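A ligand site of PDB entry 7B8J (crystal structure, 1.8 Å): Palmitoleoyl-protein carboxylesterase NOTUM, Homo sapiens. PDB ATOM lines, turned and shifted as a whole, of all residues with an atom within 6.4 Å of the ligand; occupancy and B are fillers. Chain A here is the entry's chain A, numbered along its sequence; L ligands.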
ATOM      1  N   GLY A  49     -10.789  21.639 -19.288  1.00  0.00           N
ATOM      2  CA  GLY A  49     -10.048  21.176 -20.442  1.00  0.00           C
ATOM      3  C   GLY A  49      -8.615  20.776 -20.107  1.00  0.00           C
ATOM      4  O   GLY A  49      -8.217  20.683 -18.946  1.00  0.00           O
ATOM      5  N   GLY A  50      -7.830  20.523 -21.169  1.00  0.00           N
ATOM      6  CA  GLY A  50      -6.414  20.207 -21.013  1.00  0.00           C
ATOM      7  C   GLY A  50      -5.856  19.097 -21.898  1.00  0.00           C
ATOM      8  O   GLY A  50      -5.166  18.189 -21.399  1.00  0.00           O
ATOM      9  N   TRP A  51      -6.120  19.159 -23.202  1.00  0.00           N
ATOM     10  CA  TRP A  51      -5.566  18.215 -24.220  1.00  0.00           C
ATOM     11  C   TRP A  51      -6.088  16.798 -23.922  1.00  0.00           C
ATOM     12  O   TRP A  51      -7.247  16.641 -23.514  1.00  0.00           O
ATOM     13  CB  TRP A  51      -4.018  18.374 -24.276  1.00  0.00           C
ATOM     14  CG  TRP A  51      -3.615  19.682 -24.931  1.00  0.00           C
ATOM     15  CD1 TRP A  51      -3.217  20.832 -24.304  1.00  0.00           C
ATOM     16  CD2 TRP A  51      -3.554  19.963 -26.338  1.00  0.00           C
ATOM     17  NE1 TRP A  51      -2.946  21.811 -25.225  1.00  0.00           N
ATOM     18  CE2 TRP A  51      -3.147  21.310 -26.485  1.00  0.00           C
ATOM     19  CE3 TRP A  51      -3.838  19.213 -27.490  1.00  0.00           C
ATOM     20  CZ2 TRP A  51      -2.983  21.913 -27.735  1.00  0.00           C
ATOM     21  CZ3 TRP A  51      -3.682  19.819 -28.740  1.00  0.00           C
ATOM     22  CH2 TRP A  51      -3.265  21.154 -28.844  1.00  0.00           C
ATOM     23  N   TYR A  52      -5.275  15.752 -24.158  1.00  0.00           N
ATOM     24  CA  TYR A  52      -5.657  14.348 -24.045  1.00  0.00           C
ATOM     25  C   TYR A  52      -4.422  13.476 -24.222  1.00  0.00           C
ATOM     26  O   TYR A  52      -3.344  13.998 -24.518  1.00  0.00           O
ATOM     27  CB  TYR A  52      -6.701  13.965 -25.098  1.00  0.00           C
ATOM     28  CG  TYR A  52      -6.284  14.232 -26.529  1.00  0.00           C
ATOM     29  CD1 TYR A  52      -5.754  13.224 -27.312  1.00  0.00           C
ATOM     30  CD2 TYR A  52      -6.472  15.490 -27.104  1.00  0.00           C
ATOM     31  CE1 TYR A  52      -5.356  13.466 -28.628  1.00  0.00           C
ATOM     32  CE2 TYR A  52      -6.090  15.741 -28.404  1.00  0.00           C
ATOM     33  CZ  TYR A  52      -5.532  14.717 -29.169  1.00  0.00           C
ATOM     34  OH  TYR A  52      -5.142  14.941 -30.474  1.00  0.00           O
ATOM     35  N   TYR A 105     -11.244  17.600 -15.060  1.00  0.00           N
ATOM     36  CA  TYR A 105     -10.947  16.732 -16.200  1.00  0.00           C
ATOM     37  C   TYR A 105      -9.821  15.779 -15.779  1.00  0.00           C
ATOM     38  O   TYR A 105      -8.670  16.187 -15.671  1.00  0.00           O
ATOM     39  CB  TYR A 105     -10.558  17.607 -17.390  1.00  0.00           C
ATOM     40  CG  TYR A 105     -10.149  16.921 -18.678  1.00  0.00           C
ATOM     41  CD1 TYR A 105     -10.884  15.854 -19.204  1.00  0.00           C
ATOM     42  CD2 TYR A 105      -9.109  17.441 -19.451  1.00  0.00           C
ATOM     43  CE1 TYR A 105     -10.523  15.269 -20.445  1.00  0.00           C
ATOM     44  CE2 TYR A 105      -8.749  16.864 -20.649  1.00  0.00           C
ATOM     45  CZ  TYR A 105      -9.465  15.785 -21.156  1.00  0.00           C
ATOM     46  OH  TYR A 105      -9.098  15.227 -22.364  1.00  0.00           O
ATOM     47  N   VAL A 110     -11.111  13.652 -23.832  1.00  0.00           N
ATOM     48  CA  VAL A 110     -11.952  14.722 -24.373  1.00  0.00           C
ATOM     49  C   VAL A 110     -13.402  14.434 -23.930  1.00  0.00           C
ATOM     50  O   VAL A 110     -14.390  14.758 -24.609  1.00  0.00           O
ATOM     51  CB  VAL A 110     -11.790  14.830 -25.915  1.00  0.00           C
ATOM     52  CG1 VAL A 110     -12.659  15.934 -26.550  1.00  0.00           C
ATOM     53  CG2 VAL A 110     -10.291  14.867 -26.362  1.00  0.00           C
ATOM     54  N   SER A 154     -14.550  24.528 -21.434  1.00  0.00           N
ATOM     55  CA  SER A 154     -13.514  25.257 -22.150  1.00  0.00           C
ATOM     56  C   SER A 154     -12.504  24.271 -22.723  1.00  0.00           C
ATOM     57  O   SER A 154     -12.095  23.335 -22.042  1.00  0.00           O
ATOM     58  CB  SER A 154     -12.801  26.268 -21.223  1.00  0.00           C
ATOM     59  OG  SER A 154     -13.663  27.288 -20.745  1.00  0.00           O
ATOM     60  N   SER A 155     -12.089  24.509 -23.977  1.00  0.00           N
ATOM     61  CA  SER A 155     -11.053  23.743 -24.651  1.00  0.00           C
ATOM     62  C   SER A 155     -11.511  22.311 -24.868  1.00  0.00           C
ATOM     63  O   SER A 155     -12.580  22.084 -25.451  1.00  0.00           O
ATOM     64  CB  SER A 155      -9.745  23.762 -23.856  1.00  0.00           C
ATOM     65  OG  SER A 155      -9.220  25.071 -23.796  1.00  0.00           O
ATOM     66  N   ALA A 156     -10.747  21.329 -24.381  1.00  0.00           N
ATOM     67  CA  ALA A 156     -11.218  19.948 -24.442  1.00  0.00           C
ATOM     68  C   ALA A 156     -12.576  19.791 -23.755  1.00  0.00           C
ATOM     69  O   ALA A 156     -13.385  18.937 -24.162  1.00  0.00           O
ATOM     70  CB  ALA A 156     -10.177  18.999 -23.826  1.00  0.00           C
ATOM     71  N   GLY A 157     -12.864  20.615 -22.741  1.00  0.00           N
ATOM     72  CA  GLY A 157     -14.184  20.583 -22.132  1.00  0.00           C
ATOM     73  C   GLY A 157     -15.251  21.193 -23.023  1.00  0.00           C
ATOM     74  O   GLY A 157     -16.420  20.801 -22.964  1.00  0.00           O
ATOM     75  N   THR A 159     -15.231  20.858 -26.376  1.00  0.00           N
ATOM     76  CA  THR A 159     -15.598  19.746 -27.266  1.00  0.00           C
ATOM     77  C   THR A 159     -16.448  18.737 -26.508  1.00  0.00           C
ATOM     78  O   THR A 159     -17.406  18.173 -27.065  1.00  0.00           O
ATOM     79  CB  THR A 159     -14.338  19.078 -27.852  1.00  0.00           C
ATOM     80  OG1 THR A 159     -13.451  20.081 -28.385  1.00  0.00           O
ATOM     81  CG2 THR A 159     -14.714  18.068 -28.932  1.00  0.00           C
ATOM     82  N   SER A 188     -14.088  27.523 -26.935  1.00  0.00           N
ATOM     83  CA  SER A 188     -12.760  27.145 -27.443  1.00  0.00           C
ATOM     84  C   SER A 188     -12.647  25.651 -27.760  1.00  0.00           C
ATOM     85  O   SER A 188     -11.572  25.043 -27.628  1.00  0.00           O
ATOM     86  CB  SER A 188     -11.643  27.560 -26.463  1.00  0.00           C
ATOM     87  OG  SER A 188     -11.554  28.971 -26.360  1.00  0.00           O
ATOM     88  N   GLY A 189     -13.745  25.049 -28.224  1.00  0.00           N
ATOM     89  CA  GLY A 189     -13.754  23.631 -28.550  1.00  0.00           C
ATOM     90  C   GLY A 189     -14.175  23.322 -29.980  1.00  0.00           C
ATOM     91  O   GLY A 189     -14.482  22.165 -30.297  1.00  0.00           O
ATOM     92  N   PHE A 191     -13.022  23.172 -33.616  1.00  0.00           N
ATOM     93  CA  PHE A 191     -11.801  23.041 -34.407  1.00  0.00           C
ATOM     94  C   PHE A 191     -12.072  22.631 -35.852  1.00  0.00           C
ATOM     95  O   PHE A 191     -13.130  22.105 -36.195  1.00  0.00           O
ATOM     96  CB  PHE A 191     -10.833  22.046 -33.751  1.00  0.00           C
ATOM     97  CG  PHE A 191     -10.412  22.467 -32.391  1.00  0.00           C
ATOM     98  CD1 PHE A 191     -11.030  21.974 -31.269  1.00  0.00           C
ATOM     99  CD2 PHE A 191      -9.415  23.409 -32.243  1.00  0.00           C
ATOM    100  CE1 PHE A 191     -10.658  22.394 -30.030  1.00  0.00           C
ATOM    101  CE2 PHE A 191      -9.027  23.833 -30.986  1.00  0.00           C
ATOM    102  CZ  PHE A 191      -9.649  23.314 -29.881  1.00  0.00           C
ATOM    103  N   ILE A 214      -6.745  11.416 -32.882  1.00  0.00           N
ATOM    104  CA  ILE A 214      -8.108  11.226 -32.377  1.00  0.00           C
ATOM    105  C   ILE A 214      -8.657   9.872 -32.818  1.00  0.00           C
ATOM    106  O   ILE A 214      -9.360   9.198 -32.058  1.00  0.00           O
ATOM    107  CB  ILE A 214      -9.011  12.379 -32.838  1.00  0.00           C
ATOM    108  CG1 ILE A 214      -8.483  13.671 -32.235  1.00  0.00           C
ATOM    109  CG2 ILE A 214     -10.462  12.123 -32.434  1.00  0.00           C
ATOM    110  CD1 ILE A 214      -8.739  13.711 -30.758  1.00  0.00           C
ATOM    111  N   TRP A 221      -9.745   4.494 -25.971  1.00  0.00           N
ATOM    112  CA  TRP A 221     -10.616   4.911 -24.875  1.00  0.00           C
ATOM    113  C   TRP A 221     -11.961   4.208 -24.881  1.00  0.00           C
ATOM    114  O   TRP A 221     -12.740   4.408 -23.929  1.00  0.00           O
ATOM    115  CB  TRP A 221     -10.917   6.415 -24.960  1.00  0.00           C
ATOM    116  CG  TRP A 221      -9.736   7.361 -25.140  1.00  0.00           C
ATOM    117  CD1 TRP A 221      -8.481   7.243 -24.610  1.00  0.00           C
ATOM    118  CD2 TRP A 221      -9.740   8.549 -25.935  1.00  0.00           C
ATOM    119  NE1 TRP A 221      -7.702   8.312 -25.008  1.00  0.00           N
ATOM    120  CE2 TRP A 221      -8.454   9.124 -25.833  1.00  0.00           C
ATOM    121  CE3 TRP A 221     -10.708   9.199 -26.718  1.00  0.00           C
ATOM    122  CZ2 TRP A 221      -8.100  10.304 -26.487  1.00  0.00           C
ATOM    123  CZ3 TRP A 221     -10.358  10.372 -27.378  1.00  0.00           C
ATOM    124  CH2 TRP A 221      -9.064  10.914 -27.259  1.00  0.00           C
ATOM    125  N   TRP A 239     -14.436   9.616 -35.507  1.00  0.00           N
ATOM    126  CA  TRP A 239     -13.581  10.769 -35.242  1.00  0.00           C
ATOM    127  C   TRP A 239     -14.182  12.062 -35.777  1.00  0.00           C
ATOM    128  O   TRP A 239     -13.940  13.142 -35.231  1.00  0.00           O
ATOM    129  CB  TRP A 239     -12.171  10.560 -35.826  1.00  0.00           C
ATOM    130  CG  TRP A 239     -12.124  10.489 -37.342  1.00  0.00           C
ATOM    131  CD1 TRP A 239     -12.179   9.370 -38.112  1.00  0.00           C
ATOM    132  CD2 TRP A 239     -12.011  11.598 -38.242  1.00  0.00           C
ATOM    133  NE1 TRP A 239     -12.112   9.717 -39.447  1.00  0.00           N
ATOM    134  CE2 TRP A 239     -12.005  11.079 -39.558  1.00  0.00           C
ATOM    135  CE3 TRP A 239     -11.911  12.992 -38.074  1.00  0.00           C
ATOM    136  CZ2 TRP A 239     -11.919  11.888 -40.695  1.00  0.00           C
ATOM    137  CZ3 TRP A 239     -11.835  13.799 -39.202  1.00  0.00           C
ATOM    138  CH2 TRP A 239     -11.834  13.240 -40.498  1.00  0.00           C
ATOM    139  N   PHE A 242     -15.983  14.636 -33.422  1.00  0.00           N
ATOM    140  CA  PHE A 242     -15.197  15.510 -32.551  1.00  0.00           C
ATOM    141  C   PHE A 242     -15.000  16.901 -33.128  1.00  0.00           C
ATOM    142  O   PHE A 242     -14.401  17.758 -32.454  1.00  0.00           O
ATOM    143  CB  PHE A 242     -13.831  14.864 -32.263  1.00  0.00           C
ATOM    144  CG  PHE A 242     -13.870  13.780 -31.220  1.00  0.00           C
ATOM    145  CD1 PHE A 242     -14.513  12.576 -31.466  1.00  0.00           C
ATOM    146  CD2 PHE A 242     -13.242  13.966 -29.993  1.00  0.00           C
ATOM    147  CE1 PHE A 242     -14.563  11.579 -30.488  1.00  0.00           C
ATOM    148  CE2 PHE A 242     -13.264  12.963 -29.026  1.00  0.00           C
ATOM    149  CZ  PHE A 242     -13.924  11.772 -29.278  1.00  0.00           C
ATOM    150  N   PHE A 243     -15.469  17.165 -34.346  1.00  0.00           N
ATOM    151  CA  PHE A 243     -15.253  18.454 -35.003  1.00  0.00           C
ATOM    152  C   PHE A 243     -16.566  19.222 -35.060  1.00  0.00           C
ATOM    153  O   PHE A 243     -17.528  18.764 -35.694  1.00  0.00           O
ATOM    154  CB  PHE A 243     -14.653  18.246 -36.391  1.00  0.00           C
ATOM    155  CG  PHE A 243     -13.206  17.853 -36.319  1.00  0.00           C
ATOM    156  CD1 PHE A 243     -12.863  16.519 -36.196  1.00  0.00           C
ATOM    157  CD2 PHE A 243     -12.222  18.819 -36.280  1.00  0.00           C
ATOM    158  CE1 PHE A 243     -11.542  16.148 -36.060  1.00  0.00           C
ATOM    159  CE2 PHE A 243     -10.877  18.452 -36.149  1.00  0.00           C
ATOM    160  CZ  PHE A 243     -10.546  17.121 -36.038  1.00  0.00           C
ATOM    161  N   ASP A 263      -7.566  30.572 -32.770  1.00  0.00           N
ATOM    162  CA  ASP A 263      -7.381  29.879 -31.499  1.00  0.00           C
ATOM    163  C   ASP A 263      -5.952  29.344 -31.393  1.00  0.00           C
ATOM    164  O   ASP A 263      -5.430  28.742 -32.342  1.00  0.00           O
ATOM    165  CB  ASP A 263      -8.399  28.735 -31.397  1.00  0.00           C
ATOM    166  CG  ASP A 263      -8.365  28.036 -30.063  1.00  0.00           C
ATOM    167  OD1 ASP A 263      -9.265  28.296 -29.241  1.00  0.00           O
ATOM    168  OD2 ASP A 263      -7.451  27.223 -29.822  1.00  0.00           O
ATOM    169  N   ALA A 265      -4.649  26.892 -29.740  1.00  0.00           N
ATOM    170  CA  ALA A 265      -4.492  25.444 -29.868  1.00  0.00           C
ATOM    171  C   ALA A 265      -4.728  24.983 -31.292  1.00  0.00           C
ATOM    172  O   ALA A 265      -4.094  24.015 -31.744  1.00  0.00           O
ATOM    173  CB  ALA A 265      -5.436  24.723 -28.895  1.00  0.00           C
ATOM    174  N   VAL A 269      -1.794  22.935 -33.413  1.00  0.00           N
ATOM    175  CA  VAL A 269      -1.932  21.711 -34.185  1.00  0.00           C
ATOM    176  C   VAL A 269      -1.671  21.943 -35.671  1.00  0.00           C
ATOM    177  O   VAL A 269      -1.392  20.979 -36.401  1.00  0.00           O
ATOM    178  CB  VAL A 269      -3.306  21.031 -33.971  1.00  0.00           C
ATOM    179  CG1 VAL A 269      -3.486  20.648 -32.511  1.00  0.00           C
ATOM    180  CG2 VAL A 269      -4.449  21.917 -34.454  1.00  0.00           C
ATOM    181  N   HIS A 312      -6.865  31.765 -26.194  1.00  0.00           N
ATOM    182  CA  HIS A 312      -7.407  30.430 -25.931  1.00  0.00           C
ATOM    183  C   HIS A 312      -8.179  30.458 -24.615  1.00  0.00           C
ATOM    184  O   HIS A 312      -7.662  30.964 -23.620  1.00  0.00           O
ATOM    185  CB  HIS A 312      -6.288  29.371 -25.879  1.00  0.00           C
ATOM    186  CG  HIS A 312      -6.803  27.964 -25.930  1.00  0.00           C
ATOM    187  ND1 HIS A 312      -7.616  27.517 -26.945  1.00  0.00           N
ATOM    188  CD2 HIS A 312      -6.630  26.912 -25.094  1.00  0.00           C
ATOM    189  CE1 HIS A 312      -7.915  26.243 -26.738  1.00  0.00           C
ATOM    190  NE2 HIS A 312      -7.328  25.852 -25.620  1.00  0.00           N
ATOM    191  N   GLU A 313      -9.408  29.931 -24.624  1.00  0.00           N
ATOM    192  CA  GLU A 313     -10.367  29.919 -23.509  1.00  0.00           C
ATOM    193  C   GLU A 313     -10.831  31.333 -23.122  1.00  0.00           C
ATOM    194  O   GLU A 313     -10.133  32.300 -23.423  1.00  0.00           O
ATOM    195  CB  GLU A 313      -9.771  29.238 -22.282  1.00  0.00           C
ATOM    196  CG  GLU A 313      -9.365  27.801 -22.512  1.00  0.00           C
ATOM    197  CD  GLU A 313      -8.822  27.141 -21.256  1.00  0.00           C
ATOM    198  OE1 GLU A 313      -8.197  27.822 -20.415  1.00  0.00           O
ATOM    199  OE2 GLU A 313      -9.037  25.919 -21.120  1.00  0.00           O
HETATM  200  C1  LIG L   1      -6.837  22.387 -26.060  1.00  0.00           C
HETATM  201  C2  LIG L   1      -6.917  22.246 -24.536  1.00  0.00           C
HETATM  202  O1  LIG L   1      -7.595  21.316 -24.034  1.00  0.00           O
HETATM  203  C3  LIG L   1      -9.001  19.448 -28.399  1.00  0.00           C
HETATM  204  C4  LIG L   1      -7.637  19.320 -28.211  1.00  0.00           C
HETATM  205  C5  LIG L   1      -6.954  20.264 -27.460  1.00  0.00           C
HETATM  206  C6  LIG L   1      -7.609  21.343 -26.886  1.00  0.00           C
HETATM  207  C7  LIG L   1      -8.964  21.477 -27.105  1.00  0.00           C
HETATM  208  C8  LIG L   1      -9.657  20.531 -27.848  1.00  0.00           C
HETATM  209  C9  LIG L   1     -11.076  16.871 -30.951  1.00  0.00           C
HETATM  210  C10 LIG L   1      -9.431  17.187 -29.193  1.00  0.00           C
HETATM  211  C11 LIG L   1      -9.681  18.548 -29.206  1.00  0.00           C
HETATM  212  C12 LIG L   1     -10.142  16.377 -30.056  1.00  0.00           C
HETATM  213  C13 LIG L   1     -10.603  19.043 -30.110  1.00  0.00           C
HETATM  214  C14 LIG L   1     -11.308  18.227 -30.988  1.00  0.00           C
HETATM  215  O2  LIG L   1      -6.309  23.081 -23.789  1.00  0.00           O
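An oxygen (O1) of the ligand lies within hydrogen-bond range of the backbone NH (N) of Ala 156 (3.2 Å). N of Trp 51 is in hydrogen-bond range of O1 of the ligand. NE2 of His 312 lies within hydrogen-bond range of O2 of the ligand (3.5 Å). N of Gly 50 is in hydrogen-bond range of O1 of the ligand (3.0 Å).
OE2 of Glu 313 sits at hydrogen-bond distance from OG of Ser 155, at 2.8 Å. The side-chain carboxylate (OD2) of Asp 263 sits at hydrogen-bond distance from a ring nitrogen (ND1) of His 312 (2.9 Å). The backbone NH of Val 110 sits at hydrogen-bond distance from the side-chain hydroxyl of Tyr 105. O of Gly 189 sits at hydrogen-bond distance from OG1 of Thr 159. The side-chain hydroxyl (OG) of Ser 155 lies within hydrogen-bond range of a ring nitrogen (NE2) of His 312, 2.7 Å away. N of Ala 265 lies within hydrogen-bond range of OD2 of Asp 263 (2.8 Å). The backbone carbonyl oxygen (O) of Trp 51 sits at hydrogen-bond distance from the side-chain hydroxyl (OH) of Tyr 105 (2.6 Å).
Tyr 52 touches the ligand (CE2 to C10, 3.7 Å). CG2 of Val 110 touches C10 of the ligand (3.8 Å). CB of Ser 155 touches O1 of the ligand, at 3.3 Å. OG1 of Thr 159 touches C13 of the ligand (3.5 Å). CE1 of Phe 191 touches C8 of the ligand, 3.0 Å away. Ile 214 touches the ligand. Phe 242 touches the ligand (O to C14, 3.5 Å). CB of Ala 265 touches C1 of the ligand (3.9 Å). Hydrophobic or aromatic side chains within 4 Å of the ligand: Trp 51, Tyr 52, Val 110, Ala 156, Phe 191, Ile 214, Phe 242 and Ala 265. 12 residues have an atom within 4 Å of the ligand: Gly 50, Trp 51, Tyr 52, Val 110, Ser 155, Ala 156, Thr 159, Phe 191, Ile 214, Phe 242, Ala 265 and His 312. The nearest printed residue that does not touch the ligand is Gly 49 (4.1 Å).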
